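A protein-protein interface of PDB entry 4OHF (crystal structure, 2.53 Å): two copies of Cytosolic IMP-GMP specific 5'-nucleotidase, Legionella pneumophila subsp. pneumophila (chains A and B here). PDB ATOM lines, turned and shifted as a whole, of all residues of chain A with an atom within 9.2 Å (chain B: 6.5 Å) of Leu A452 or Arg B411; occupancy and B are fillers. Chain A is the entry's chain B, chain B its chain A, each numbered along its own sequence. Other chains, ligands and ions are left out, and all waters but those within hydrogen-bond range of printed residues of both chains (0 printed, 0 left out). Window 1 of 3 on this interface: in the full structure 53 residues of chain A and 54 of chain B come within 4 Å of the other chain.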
ATOM      1  N   ALA A 448      13.698  15.853  21.760  1.00  0.00           N
ATOM      2  CA  ALA A 448      14.029  15.653  23.156  1.00  0.00           C
ATOM      3  C   ALA A 448      13.795  14.207  23.554  1.00  0.00           C
ATOM      4  O   ALA A 448      12.862  13.564  23.071  1.00  0.00           O
ATOM      5  CB  ALA A 448      13.186  16.553  24.008  1.00  0.00           C
ATOM      6  N   ASN A 449      14.650  13.693  24.426  1.00  0.00           N
ATOM      7  CA  ASN A 449      14.501  12.332  24.916  1.00  0.00           C
ATOM      8  C   ASN A 449      13.331  12.405  25.886  1.00  0.00           C
ATOM      9  O   ASN A 449      13.202  13.395  26.605  1.00  0.00           O
ATOM     10  CB  ASN A 449      15.757  11.909  25.667  1.00  0.00           C
ATOM     11  CG  ASN A 449      17.013  12.026  24.820  1.00  0.00           C
ATOM     12  OD1 ASN A 449      18.115  12.229  25.344  1.00  0.00           O
ATOM     13  ND2 ASN A 449      16.858  11.885  23.501  1.00  0.00           N
ATOM     14  N   ARG A 450      12.475  11.383  25.911  1.00  0.00           N
ATOM     15  CA  ARG A 450      11.325  11.387  26.828  1.00  0.00           C
ATOM     16  C   ARG A 450      11.775  11.704  28.252  1.00  0.00           C
ATOM     17  O   ARG A 450      12.830  11.251  28.692  1.00  0.00           O
ATOM     18  CB  ARG A 450      10.622  10.023  26.838  1.00  0.00           C
ATOM     19  CG  ARG A 450       9.283   9.949  26.116  1.00  0.00           C
ATOM     20  CD  ARG A 450       8.491   8.760  26.642  1.00  0.00           C
ATOM     21  NE  ARG A 450       9.353   7.599  26.870  1.00  0.00           N
ATOM     22  CZ  ARG A 450       8.972   6.486  27.497  1.00  0.00           C
ATOM     23  NH1 ARG A 450       7.729   6.375  27.962  1.00  0.00           N
ATOM     24  NH2 ARG A 450       9.833   5.487  27.671  1.00  0.00           N
ATOM     25  N   ARG A 451      10.970  12.467  28.977  1.00  0.00           N
ATOM     26  CA  ARG A 451      11.314  12.820  30.348  1.00  0.00           C
ATOM     27  C   ARG A 451      10.810  11.769  31.348  1.00  0.00           C
ATOM     28  O   ARG A 451      11.268  11.727  32.497  1.00  0.00           O
ATOM     29  CB  ARG A 451      10.749  14.207  30.693  1.00  0.00           C
ATOM     30  N   LEU A 452       9.882  10.918  30.912  1.00  0.00           N
ATOM     31  CA  LEU A 452       9.317   9.871  31.775  1.00  0.00           C
ATOM     32  C   LEU A 452       8.516  10.381  32.991  1.00  0.00           C
ATOM     33  O   LEU A 452       9.063  10.973  33.926  1.00  0.00           O
ATOM     34  CB  LEU A 452      10.419   8.931  32.268  1.00  0.00           C
ATOM     35  CG  LEU A 452      11.038   7.920  31.296  1.00  0.00           C
ATOM     36  CD1 LEU A 452      12.052   7.077  32.073  1.00  0.00           C
ATOM     37  CD2 LEU A 452       9.967   7.022  30.676  1.00  0.00           C
ATOM     38  N   LEU A 453       7.211  10.137  32.958  1.00  0.00           N
ATOM     39  CA  LEU A 453       6.308  10.539  34.019  1.00  0.00           C
ATOM     40  C   LEU A 453       6.274   9.431  35.064  1.00  0.00           C
ATOM     41  O   LEU A 453       6.478   8.267  34.733  1.00  0.00           O
ATOM     42  CB  LEU A 453       4.915  10.743  33.436  1.00  0.00           C
ATOM     43  CG  LEU A 453       4.767  11.888  32.443  1.00  0.00           C
ATOM     44  CD1 LEU A 453       3.415  11.813  31.755  1.00  0.00           C
ATOM     45  CD2 LEU A 453       4.929  13.202  33.186  1.00  0.00           C
ATOM     46  N   ALA A 454       6.009   9.786  36.317  1.00  0.00           N
ATOM     47  CA  ALA A 454       5.968   8.806  37.399  1.00  0.00           C
ATOM     48  C   ALA A 454       5.119   7.577  37.077  1.00  0.00           C
ATOM     49  O   ALA A 454       5.415   6.483  37.551  1.00  0.00           O
ATOM     50  CB  ALA A 454       5.483   9.468  38.695  1.00  0.00           C
ATOM     51  N   HIS A 455       4.070   7.735  36.274  1.00  0.00           N
ATOM     52  CA  HIS A 455       3.257   6.570  35.933  1.00  0.00           C
ATOM     53  C   HIS A 455       3.773   5.847  34.683  1.00  0.00           C
ATOM     54  O   HIS A 455       3.268   4.782  34.331  1.00  0.00           O
ATOM     55  CB  HIS A 455       1.768   6.939  35.772  1.00  0.00           C
ATOM     56  CG  HIS A 455       1.481   7.896  34.656  1.00  0.00           C
ATOM     57  ND1 HIS A 455       1.662   9.258  34.775  1.00  0.00           N
ATOM     58  CD2 HIS A 455       1.013   7.687  33.402  1.00  0.00           C
ATOM     59  CE1 HIS A 455       1.317   9.844  33.641  1.00  0.00           C
ATOM     60  NE2 HIS A 455       0.920   8.914  32.791  1.00  0.00           N
ATOM     61  N   ASP A 456       4.783   6.421  34.027  1.00  0.00           N
ATOM     62  CA  ASP A 456       5.384   5.813  32.839  1.00  0.00           C
ATOM     63  C   ASP A 456       6.230   4.601  33.183  1.00  0.00           C
ATOM     64  O   ASP A 456       6.986   4.614  34.155  1.00  0.00           O
ATOM     65  CB  ASP A 456       6.298   6.794  32.101  1.00  0.00           C
ATOM     66  CG  ASP A 456       5.538   7.760  31.244  1.00  0.00           C
ATOM     67  OD1 ASP A 456       4.451   7.379  30.769  1.00  0.00           O
ATOM     68  OD2 ASP A 456       6.029   8.890  31.030  1.00  0.00           O
ATOM     69  N   ILE A 457       6.115   3.562  32.365  1.00  0.00           N
ATOM     70  CA  ILE A 457       6.894   2.349  32.557  1.00  0.00           C
ATOM     71  C   ILE A 457       8.288   2.538  31.950  1.00  0.00           C
ATOM     72  O   ILE A 457       8.425   2.932  30.789  1.00  0.00           O
ATOM     73  CB  ILE A 457       6.209   1.144  31.896  1.00  0.00           C
ATOM     74  CG1 ILE A 457       4.906   0.822  32.640  1.00  0.00           C
ATOM     75  CG2 ILE A 457       7.163  -0.037  31.856  1.00  0.00           C
ATOM     76  CD1 ILE A 457       5.066   0.672  34.147  1.00  0.00           C
ATOM     77  N   ASP A 458       9.317   2.259  32.742  1.00  0.00           N
ATOM     78  CA  ASP A 458      10.699   2.415  32.301  1.00  0.00           C
ATOM     79  C   ASP A 458      11.096   1.280  31.347  1.00  0.00           C
ATOM     80  O   ASP A 458      10.622   0.150  31.483  1.00  0.00           O
ATOM     81  CB  ASP A 458      11.620   2.432  33.529  1.00  0.00           C
ATOM     82  CG  ASP A 458      12.913   3.191  33.286  1.00  0.00           C
ATOM     83  OD1 ASP A 458      12.863   4.433  33.131  1.00  0.00           O
ATOM     84  OD2 ASP A 458      13.981   2.541  33.251  1.00  0.00           O
ATOM     85  N   ILE A 459      11.960   1.581  30.382  1.00  0.00           N
ATOM     86  CA  ILE A 459      12.399   0.573  29.416  1.00  0.00           C
ATOM     87  C   ILE A 459      13.924   0.416  29.386  1.00  0.00           C
ATOM     88  O   ILE A 459      14.542   0.774  28.360  1.00  0.00           O
ATOM     89  CB  ILE A 459      11.886   0.904  27.983  1.00  0.00           C
ATOM     90  CG1 ILE A 459      12.256   2.344  27.604  1.00  0.00           C
ATOM     91  CG2 ILE A 459      10.380   0.691  27.911  1.00  0.00           C
ATOM     92  CD1 ILE A 459      11.782   2.770  26.232  1.00  0.00           C
ATOM     93  N   LYS B  83      -5.387  22.275  23.555  1.00  0.00           N
ATOM     94  CA  LYS B  83      -4.617  21.355  24.380  1.00  0.00           C
ATOM     95  C   LYS B  83      -3.224  21.985  24.493  1.00  0.00           C
ATOM     96  O   LYS B  83      -2.428  21.978  23.541  1.00  0.00           O
ATOM     97  CB  LYS B  83      -4.501  19.982  23.732  1.00  0.00           C
ATOM     98  CG  LYS B  83      -3.843  18.963  24.660  1.00  0.00           C
ATOM     99  CD  LYS B  83      -3.687  17.617  23.994  1.00  0.00           C
ATOM    100  CE  LYS B  83      -3.101  16.604  24.945  1.00  0.00           C
ATOM    101  NZ  LYS B  83      -2.665  15.388  24.220  1.00  0.00           N
ATOM    102  N   LEU B  84      -2.943  22.544  25.664  1.00  0.00           N
ATOM    103  CA  LEU B  84      -1.677  23.202  25.898  1.00  0.00           C
ATOM    104  C   LEU B  84      -0.603  22.301  26.502  1.00  0.00           C
ATOM    105  O   LEU B  84      -0.902  21.303  27.164  1.00  0.00           O
ATOM    106  CB  LEU B  84      -1.888  24.414  26.814  1.00  0.00           C
ATOM    107  CG  LEU B  84      -2.774  25.606  26.411  1.00  0.00           C
ATOM    108  CD1 LEU B  84      -2.523  25.983  24.953  1.00  0.00           C
ATOM    109  CD2 LEU B  84      -4.220  25.269  26.608  1.00  0.00           C
ATOM    110  N   GLU B 330      -5.221   5.533  30.268  1.00  0.00           N
ATOM    111  CA  GLU B 330      -3.922   6.025  29.838  1.00  0.00           C
ATOM    112  C   GLU B 330      -2.861   4.949  30.001  1.00  0.00           C
ATOM    113  O   GLU B 330      -2.076   4.729  29.092  1.00  0.00           O
ATOM    114  CB  GLU B 330      -3.509   7.257  30.644  1.00  0.00           C
ATOM    115  CG  GLU B 330      -4.112   8.572  30.191  1.00  0.00           C
ATOM    116  CD  GLU B 330      -3.201   9.357  29.273  1.00  0.00           C
ATOM    117  OE1 GLU B 330      -1.970   9.367  29.506  1.00  0.00           O
ATOM    118  OE2 GLU B 330      -3.725   9.983  28.329  1.00  0.00           O
ATOM    119  N   GLN B 334      -0.794   2.846  27.098  1.00  0.00           N
ATOM    120  CA  GLN B 334       0.652   2.962  27.021  1.00  0.00           C
ATOM    121  C   GLN B 334       1.281   1.573  27.049  1.00  0.00           C
ATOM    122  O   GLN B 334       2.307   1.323  26.416  1.00  0.00           O
ATOM    123  CB  GLN B 334       1.159   3.838  28.172  1.00  0.00           C
ATOM    124  CG  GLN B 334       0.596   5.268  28.092  1.00  0.00           C
ATOM    125  CD  GLN B 334       1.311   6.254  28.995  1.00  0.00           C
ATOM    126  OE1 GLN B 334       1.142   7.475  28.857  1.00  0.00           O
ATOM    127  NE2 GLN B 334       2.111   5.734  29.928  1.00  0.00           N
ATOM    128  N   GLU B 341       7.174   2.186  21.721  1.00  0.00           N
ATOM    129  CA  GLU B 341       8.039   3.038  22.524  1.00  0.00           C
ATOM    130  C   GLU B 341       9.459   2.488  22.520  1.00  0.00           C
ATOM    131  O   GLU B 341      10.418   3.210  22.265  1.00  0.00           O
ATOM    132  CB  GLU B 341       7.513   3.117  23.957  1.00  0.00           C
ATOM    133  CG  GLU B 341       8.167   4.211  24.790  1.00  0.00           C
ATOM    134  CD  GLU B 341       7.950   5.597  24.198  1.00  0.00           C
ATOM    135  OE1 GLU B 341       6.771   5.982  24.004  1.00  0.00           O
ATOM    136  OE2 GLU B 341       8.954   6.303  23.928  1.00  0.00           O
ATOM    137  N   TRP B 406      -7.704  13.776  20.493  1.00  0.00           N
ATOM    138  CA  TRP B 406      -6.855  14.624  21.322  1.00  0.00           C
ATOM    139  C   TRP B 406      -5.585  14.005  21.895  1.00  0.00           C
ATOM    140  O   TRP B 406      -4.851  14.668  22.629  1.00  0.00           O
ATOM    141  CB  TRP B 406      -7.667  15.210  22.473  1.00  0.00           C
ATOM    142  CG  TRP B 406      -8.811  16.100  22.062  1.00  0.00           C
ATOM    143  CD1 TRP B 406     -10.115  15.730  21.880  1.00  0.00           C
ATOM    144  CD2 TRP B 406      -8.773  17.524  21.884  1.00  0.00           C
ATOM    145  NE1 TRP B 406     -10.893  16.838  21.615  1.00  0.00           N
ATOM    146  CE2 TRP B 406     -10.094  17.950  21.612  1.00  0.00           C
ATOM    147  CE3 TRP B 406      -7.752  18.483  21.937  1.00  0.00           C
ATOM    148  CZ2 TRP B 406     -10.421  19.296  21.395  1.00  0.00           C
ATOM    149  CZ3 TRP B 406      -8.078  19.827  21.721  1.00  0.00           C
ATOM    150  CH2 TRP B 406      -9.403  20.218  21.455  1.00  0.00           C
ATOM    151  N   GLU B 407      -5.320  12.749  21.561  1.00  0.00           N
ATOM    152  CA  GLU B 407      -4.131  12.053  22.053  1.00  0.00           C
ATOM    153  C   GLU B 407      -4.141  11.861  23.575  1.00  0.00           C
ATOM    154  O   GLU B 407      -5.213  11.889  24.199  1.00  0.00           O
ATOM    155  CB  GLU B 407      -2.859  12.781  21.597  1.00  0.00           C
ATOM    156  CG  GLU B 407      -2.551  12.578  20.106  1.00  0.00           C
ATOM    157  CD  GLU B 407      -1.556  13.590  19.546  1.00  0.00           C
ATOM    158  OE1 GLU B 407      -1.270  13.517  18.324  1.00  0.00           O
ATOM    159  OE2 GLU B 407      -1.066  14.455  20.315  1.00  0.00           O
ATOM    160  N   ARG B 408      -2.963  11.661  24.173  1.00  0.00           N
ATOM    161  CA  ARG B 408      -2.888  11.418  25.615  1.00  0.00           C
ATOM    162  C   ARG B 408      -3.230  12.633  26.478  1.00  0.00           C
ATOM    163  O   ARG B 408      -3.164  13.779  26.038  1.00  0.00           O
ATOM    164  CB  ARG B 408      -1.498  10.895  26.019  1.00  0.00           C
ATOM    165  CG  ARG B 408      -0.826   9.912  25.056  1.00  0.00           C
ATOM    166  CD  ARG B 408       0.333  10.605  24.340  1.00  0.00           C
ATOM    167  NE  ARG B 408       1.521   9.764  24.145  1.00  0.00           N
ATOM    168  CZ  ARG B 408       2.113   9.031  25.089  1.00  0.00           C
ATOM    169  NH1 ARG B 408       3.197   8.317  24.801  1.00  0.00           N
ATOM    170  NH2 ARG B 408       1.612   8.981  26.316  1.00  0.00           N
ATOM    171  N   VAL B 409      -3.600  12.356  27.718  1.00  0.00           N
ATOM    172  CA  VAL B 409      -3.956  13.367  28.698  1.00  0.00           C
ATOM    173  C   VAL B 409      -2.736  14.051  29.318  1.00  0.00           C
ATOM    174  O   VAL B 409      -2.745  15.256  29.554  1.00  0.00           O
ATOM    175  CB  VAL B 409      -4.792  12.731  29.829  1.00  0.00           C
ATOM    176  CG1 VAL B 409      -4.959  13.705  30.983  1.00  0.00           C
ATOM    177  CG2 VAL B 409      -6.149  12.329  29.288  1.00  0.00           C
ATOM    178  N   PHE B 410      -1.694  13.267  29.579  1.00  0.00           N
ATOM    179  CA  PHE B 410      -0.476  13.759  30.207  1.00  0.00           C
ATOM    180  C   PHE B 410       0.579  14.280  29.229  1.00  0.00           C
ATOM    181  O   PHE B 410       1.590  14.848  29.644  1.00  0.00           O
ATOM    182  CB  PHE B 410       0.132  12.642  31.073  1.00  0.00           C
ATOM    183  CG  PHE B 410      -0.651  12.335  32.323  1.00  0.00           C
ATOM    184  CD1 PHE B 410      -0.301  12.916  33.544  1.00  0.00           C
ATOM    185  CD2 PHE B 410      -1.737  11.462  32.287  1.00  0.00           C
ATOM    186  CE1 PHE B 410      -1.015  12.632  34.713  1.00  0.00           C
ATOM    187  CE2 PHE B 410      -2.457  11.171  33.453  1.00  0.00           C
ATOM    188  CZ  PHE B 410      -2.095  11.758  34.666  1.00  0.00           C
ATOM    189  N   ARG B 411       0.350  14.094  27.935  1.00  0.00           N
ATOM    190  CA  ARG B 411       1.307  14.554  26.937  1.00  0.00           C
ATOM    191  C   ARG B 411       0.700  15.509  25.923  1.00  0.00           C
ATOM    192  O   ARG B 411      -0.364  15.247  25.374  1.00  0.00           O
ATOM    193  CB  ARG B 411       1.900  13.368  26.188  1.00  0.00           C
ATOM    194  CG  ARG B 411       3.376  13.173  26.422  1.00  0.00           C
ATOM    195  CD  ARG B 411       3.526  12.587  27.787  1.00  0.00           C
ATOM    196  NE  ARG B 411       4.866  12.230  28.097  1.00  0.00           N
ATOM    197  CZ  ARG B 411       5.425  11.071  28.422  1.00  0.00           C
ATOM    198  NH1 ARG B 411       6.720  11.159  28.649  1.00  0.00           N
ATOM    199  NH2 ARG B 411       4.807   9.889  28.520  1.00  0.00           N
ATOM    200  N   ALA B 412       1.378  16.625  25.682  1.00  0.00           N
ATOM    201  CA  ALA B 412       0.925  17.615  24.710  1.00  0.00           C
ATOM    202  C   ALA B 412       1.987  17.528  23.646  1.00  0.00           C
ATOM    203  O   ALA B 412       3.034  18.168  23.744  1.00  0.00           O
ATOM    204  CB  ALA B 412       0.904  19.000  25.319  1.00  0.00           C
ATOM    205  N   GLY B 413       1.721  16.730  22.624  1.00  0.00           N
ATOM    206  CA  GLY B 413       2.723  16.551  21.601  1.00  0.00           C
ATOM    207  C   GLY B 413       3.772  15.700  22.282  1.00  0.00           C
ATOM    208  O   GLY B 413       3.434  14.730  22.956  1.00  0.00           O
ATOM    209  N   ALA B 414       5.040  16.059  22.141  1.00  0.00           N
ATOM    210  CA  ALA B 414       6.099  15.280  22.769  1.00  0.00           C
ATOM    211  C   ALA B 414       6.284  15.672  24.227  1.00  0.00           C
ATOM    212  O   ALA B 414       6.729  14.863  25.038  1.00  0.00           O
ATOM    213  CB  ALA B 414       7.411  15.474  22.012  1.00  0.00           C
ATOM    214  N   GLU B 415       5.935  16.915  24.555  1.00  0.00           N
ATOM    215  CA  GLU B 415       6.095  17.429  25.917  1.00  0.00           C
ATOM    216  C   GLU B 415       4.971  16.968  26.825  1.00  0.00           C
ATOM    217  O   GLU B 415       3.989  16.383  26.375  1.00  0.00           O
ATOM    218  CB  GLU B 415       6.091  18.961  25.910  1.00  0.00           C
ATOM    219  CG  GLU B 415       6.770  19.620  24.717  1.00  0.00           C
ATOM    220  CD  GLU B 415       6.717  21.145  24.774  1.00  0.00           C
ATOM    221  OE1 GLU B 415       7.324  21.738  25.702  1.00  0.00           O
ATOM    222  OE2 GLU B 415       6.063  21.743  23.886  1.00  0.00           O
ATOM    223  N   GLU B 416       5.117  17.218  28.119  1.00  0.00           N
ATOM    224  CA  GLU B 416       4.042  16.880  29.027  1.00  0.00           C
ATOM    225  C   GLU B 416       3.009  17.984  28.831  1.00  0.00           C
ATOM    226  O   GLU B 416       3.348  19.106  28.456  1.00  0.00           O
ATOM    227  CB  GLU B 416       4.520  16.854  30.479  1.00  0.00           C
ATOM    228  CG  GLU B 416       5.715  17.724  30.762  1.00  0.00           C
ATOM    229  CD  GLU B 416       7.015  17.053  30.383  1.00  0.00           C
ATOM    230  OE1 GLU B 416       8.052  17.746  30.353  1.00  0.00           O
ATOM    231  OE2 GLU B 416       7.000  15.828  30.120  1.00  0.00           O
ATOM    232  N   SER B 417       1.747  17.669  29.070  1.00  0.00           N
ATOM    233  CA  SER B 417       0.687  18.646  28.910  1.00  0.00           C
ATOM    234  C   SER B 417       0.578  19.580  30.120  1.00  0.00           C
ATOM    235  O   SER B 417       1.247  19.397  31.144  1.00  0.00           O
ATOM    236  CB  SER B 417      -0.632  17.917  28.718  1.00  0.00           C
ATOM    237  OG  SER B 417      -0.894  17.123  29.857  1.00  0.00           O
ATOM    238  N   ALA B 420      -0.497  17.627  33.027  1.00  0.00           N
ATOM    239  CA  ALA B 420       0.583  16.839  33.622  1.00  0.00           C
ATOM    240  C   ALA B 420       1.365  17.703  34.606  1.00  0.00           C
ATOM    241  O   ALA B 420       1.788  17.237  35.664  1.00  0.00           O
ATOM    242  CB  ALA B 420       1.521  16.319  32.531  1.00  0.00           C
ATOM    243  N   ASN B 449      10.481   8.644  42.332  1.00  0.00           N
ATOM    244  CA  ASN B 449      11.355   7.858  41.474  1.00  0.00           C
ATOM    245  C   ASN B 449      12.690   8.557  41.285  1.00  0.00           C
ATOM    246  O   ASN B 449      12.759   9.760  41.030  1.00  0.00           O
ATOM    247  CB  ASN B 449      10.682   7.633  40.117  1.00  0.00           C
ATOM    248  CG  ASN B 449       9.706   8.749  39.765  1.00  0.00           C
ATOM    249  OD1 ASN B 449      10.106   9.877  39.454  1.00  0.00           O
ATOM    250  ND2 ASN B 449       8.414   8.442  39.837  1.00  0.00           N
ATOM    251  N   ARG B 451      14.344   8.668  38.970  1.00  0.00           N
ATOM    252  CA  ARG B 451      14.425   8.713  37.512  1.00  0.00           C
ATOM    253  C   ARG B 451      15.392   9.784  37.062  1.00  0.00           C
ATOM    254  O   ARG B 451      16.073   9.619  36.056  1.00  0.00           O
ATOM    255  CB  ARG B 451      13.041   8.985  36.902  1.00  0.00           C
ATOM    256  CG  ARG B 451      12.304   7.744  36.395  1.00  0.00           C
ATOM    257  CD  ARG B 451      10.810   8.018  36.185  1.00  0.00           C
ATOM    258  NE  ARG B 451      10.118   6.916  35.519  1.00  0.00           N
ATOM    259  CZ  ARG B 451      10.288   5.631  35.815  1.00  0.00           C
ATOM    260  NH1 ARG B 451      11.136   5.266  36.772  1.00  0.00           N
ATOM    261  NH2 ARG B 451       9.602   4.705  35.159  1.00  0.00           N
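Positions printed for both chains: 449 and 451.
Of the 13 pairs that touch across the chains among the printed residues, none has its exchanged pair printed and touching as well.
Arg A450 touches Arg B411 (CD to NH1, 3.6 Å).
Arg B411 touches Leu A452 (NH1 to N, 3.9 Å).
NE of Arg B451 touches CB of Leu A452, 3.8 Å away.
CB of Phe B410 touches CD1 of Leu A453, at 3.5 Å.
CD1 of Leu A453 touches NE of Arg B411, at 3.96 Å.
O of Leu A453 touches NE of Arg B451 (3.96 Å).
CB of Ala A454 touches ND2 of Asn B449, at 3.3 Å.
His A455 touches Phe B410 (CE1 to CG, 3.4 Å).
NE2 of Gln B334 lies within hydrogen-bond range of OD1 of Asp A456 (3.0 Å).
The side-chain carboxylate (OE2) of Glu B341 lies within salt-bridge range of the guanidinium group (NE) of Arg A450 (3.2 Å).
The guanidinium group (NH2) of Arg B411 lies within salt-bridge range of the side-chain carboxylate (OD2) of Asp A456.
NH2 of Arg B451 is in hydrogen-bond range of O of Asp A456, 2.8 Å away.
NH2 of Arg B451 is in salt-bridge range of OD1 of Asp A458.
Of the 20 printed residues of chain B, 6 touch a printed residue of chain A.
Hydrophobic or aromatic side chains of chain B that line the printed part of chain A: Phe B410.
Hydrophobic or aromatic side chains of chain A within 4 Å of the printed part of chain B: Leu A452, Leu A453, Ala A454 and His A455.
Among the printed residues, 13 pairs touch across the chains.
Among the printed residues, Asp or Glu carboxylates within 4 Å of a Lys or Arg side-chain nitrogen of the other chain: Arg A450 with Glu B341 (3.2 Å), Asp A456 with Arg B411 (3.0 Å) and Asp A458 with Arg B451 (3.8 Å).
The side-chain amino group of Lys B83 is in hydrogen-bond range of the backbone carbonyl oxygen of Arg B411 (2.6 Å).
The side-chain amide oxygen (OE1) of Gln B334 lies within hydrogen-bond range of the guanidinium group (NH2) of Arg B408 (3.0 Å).
The backbone NH (N) of Ser B417 is in hydrogen-bond range of the backbone carbonyl oxygen (O) of Phe B410 (2.9 Å).
The backbone NH of Leu A453 sits at hydrogen-bond distance from the side-chain carboxylate of Asp A456 (2.6 Å).
Leu A452 touches two residues of chain B.
Of the printed residues of chain B, His A455 touches Phe B410.
Of the printed residues of chain B, Asp A456 touches Gln B334 (3.0 Å), Arg B411 (3.0 Å) and Arg B451 (2.8 Å).
Ile A457 touches none of the printed residues of chain B.
No residue of chain A comes within 4 Å of Arg B408.
Of the printed residues of chain A, Phe B410 touches Leu A453 and His A455.
Of the printed residues of chain A, Asn B449 touches Ala A454.
Of the printed residues of chain A, Arg B451 touches Leu A452, Leu A453, Asp A456 and Asp A458.
The nearest printed residue of chain B that does not touch Leu A452 is Asn B449 (5.7 Å).
The nearest residue of chain A that does not touch Arg B411 is Arg A451 (4.5 Å).
The nearest printed residue of chain B that does not touch Asp A458 is Glu B341 (7.8 Å).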
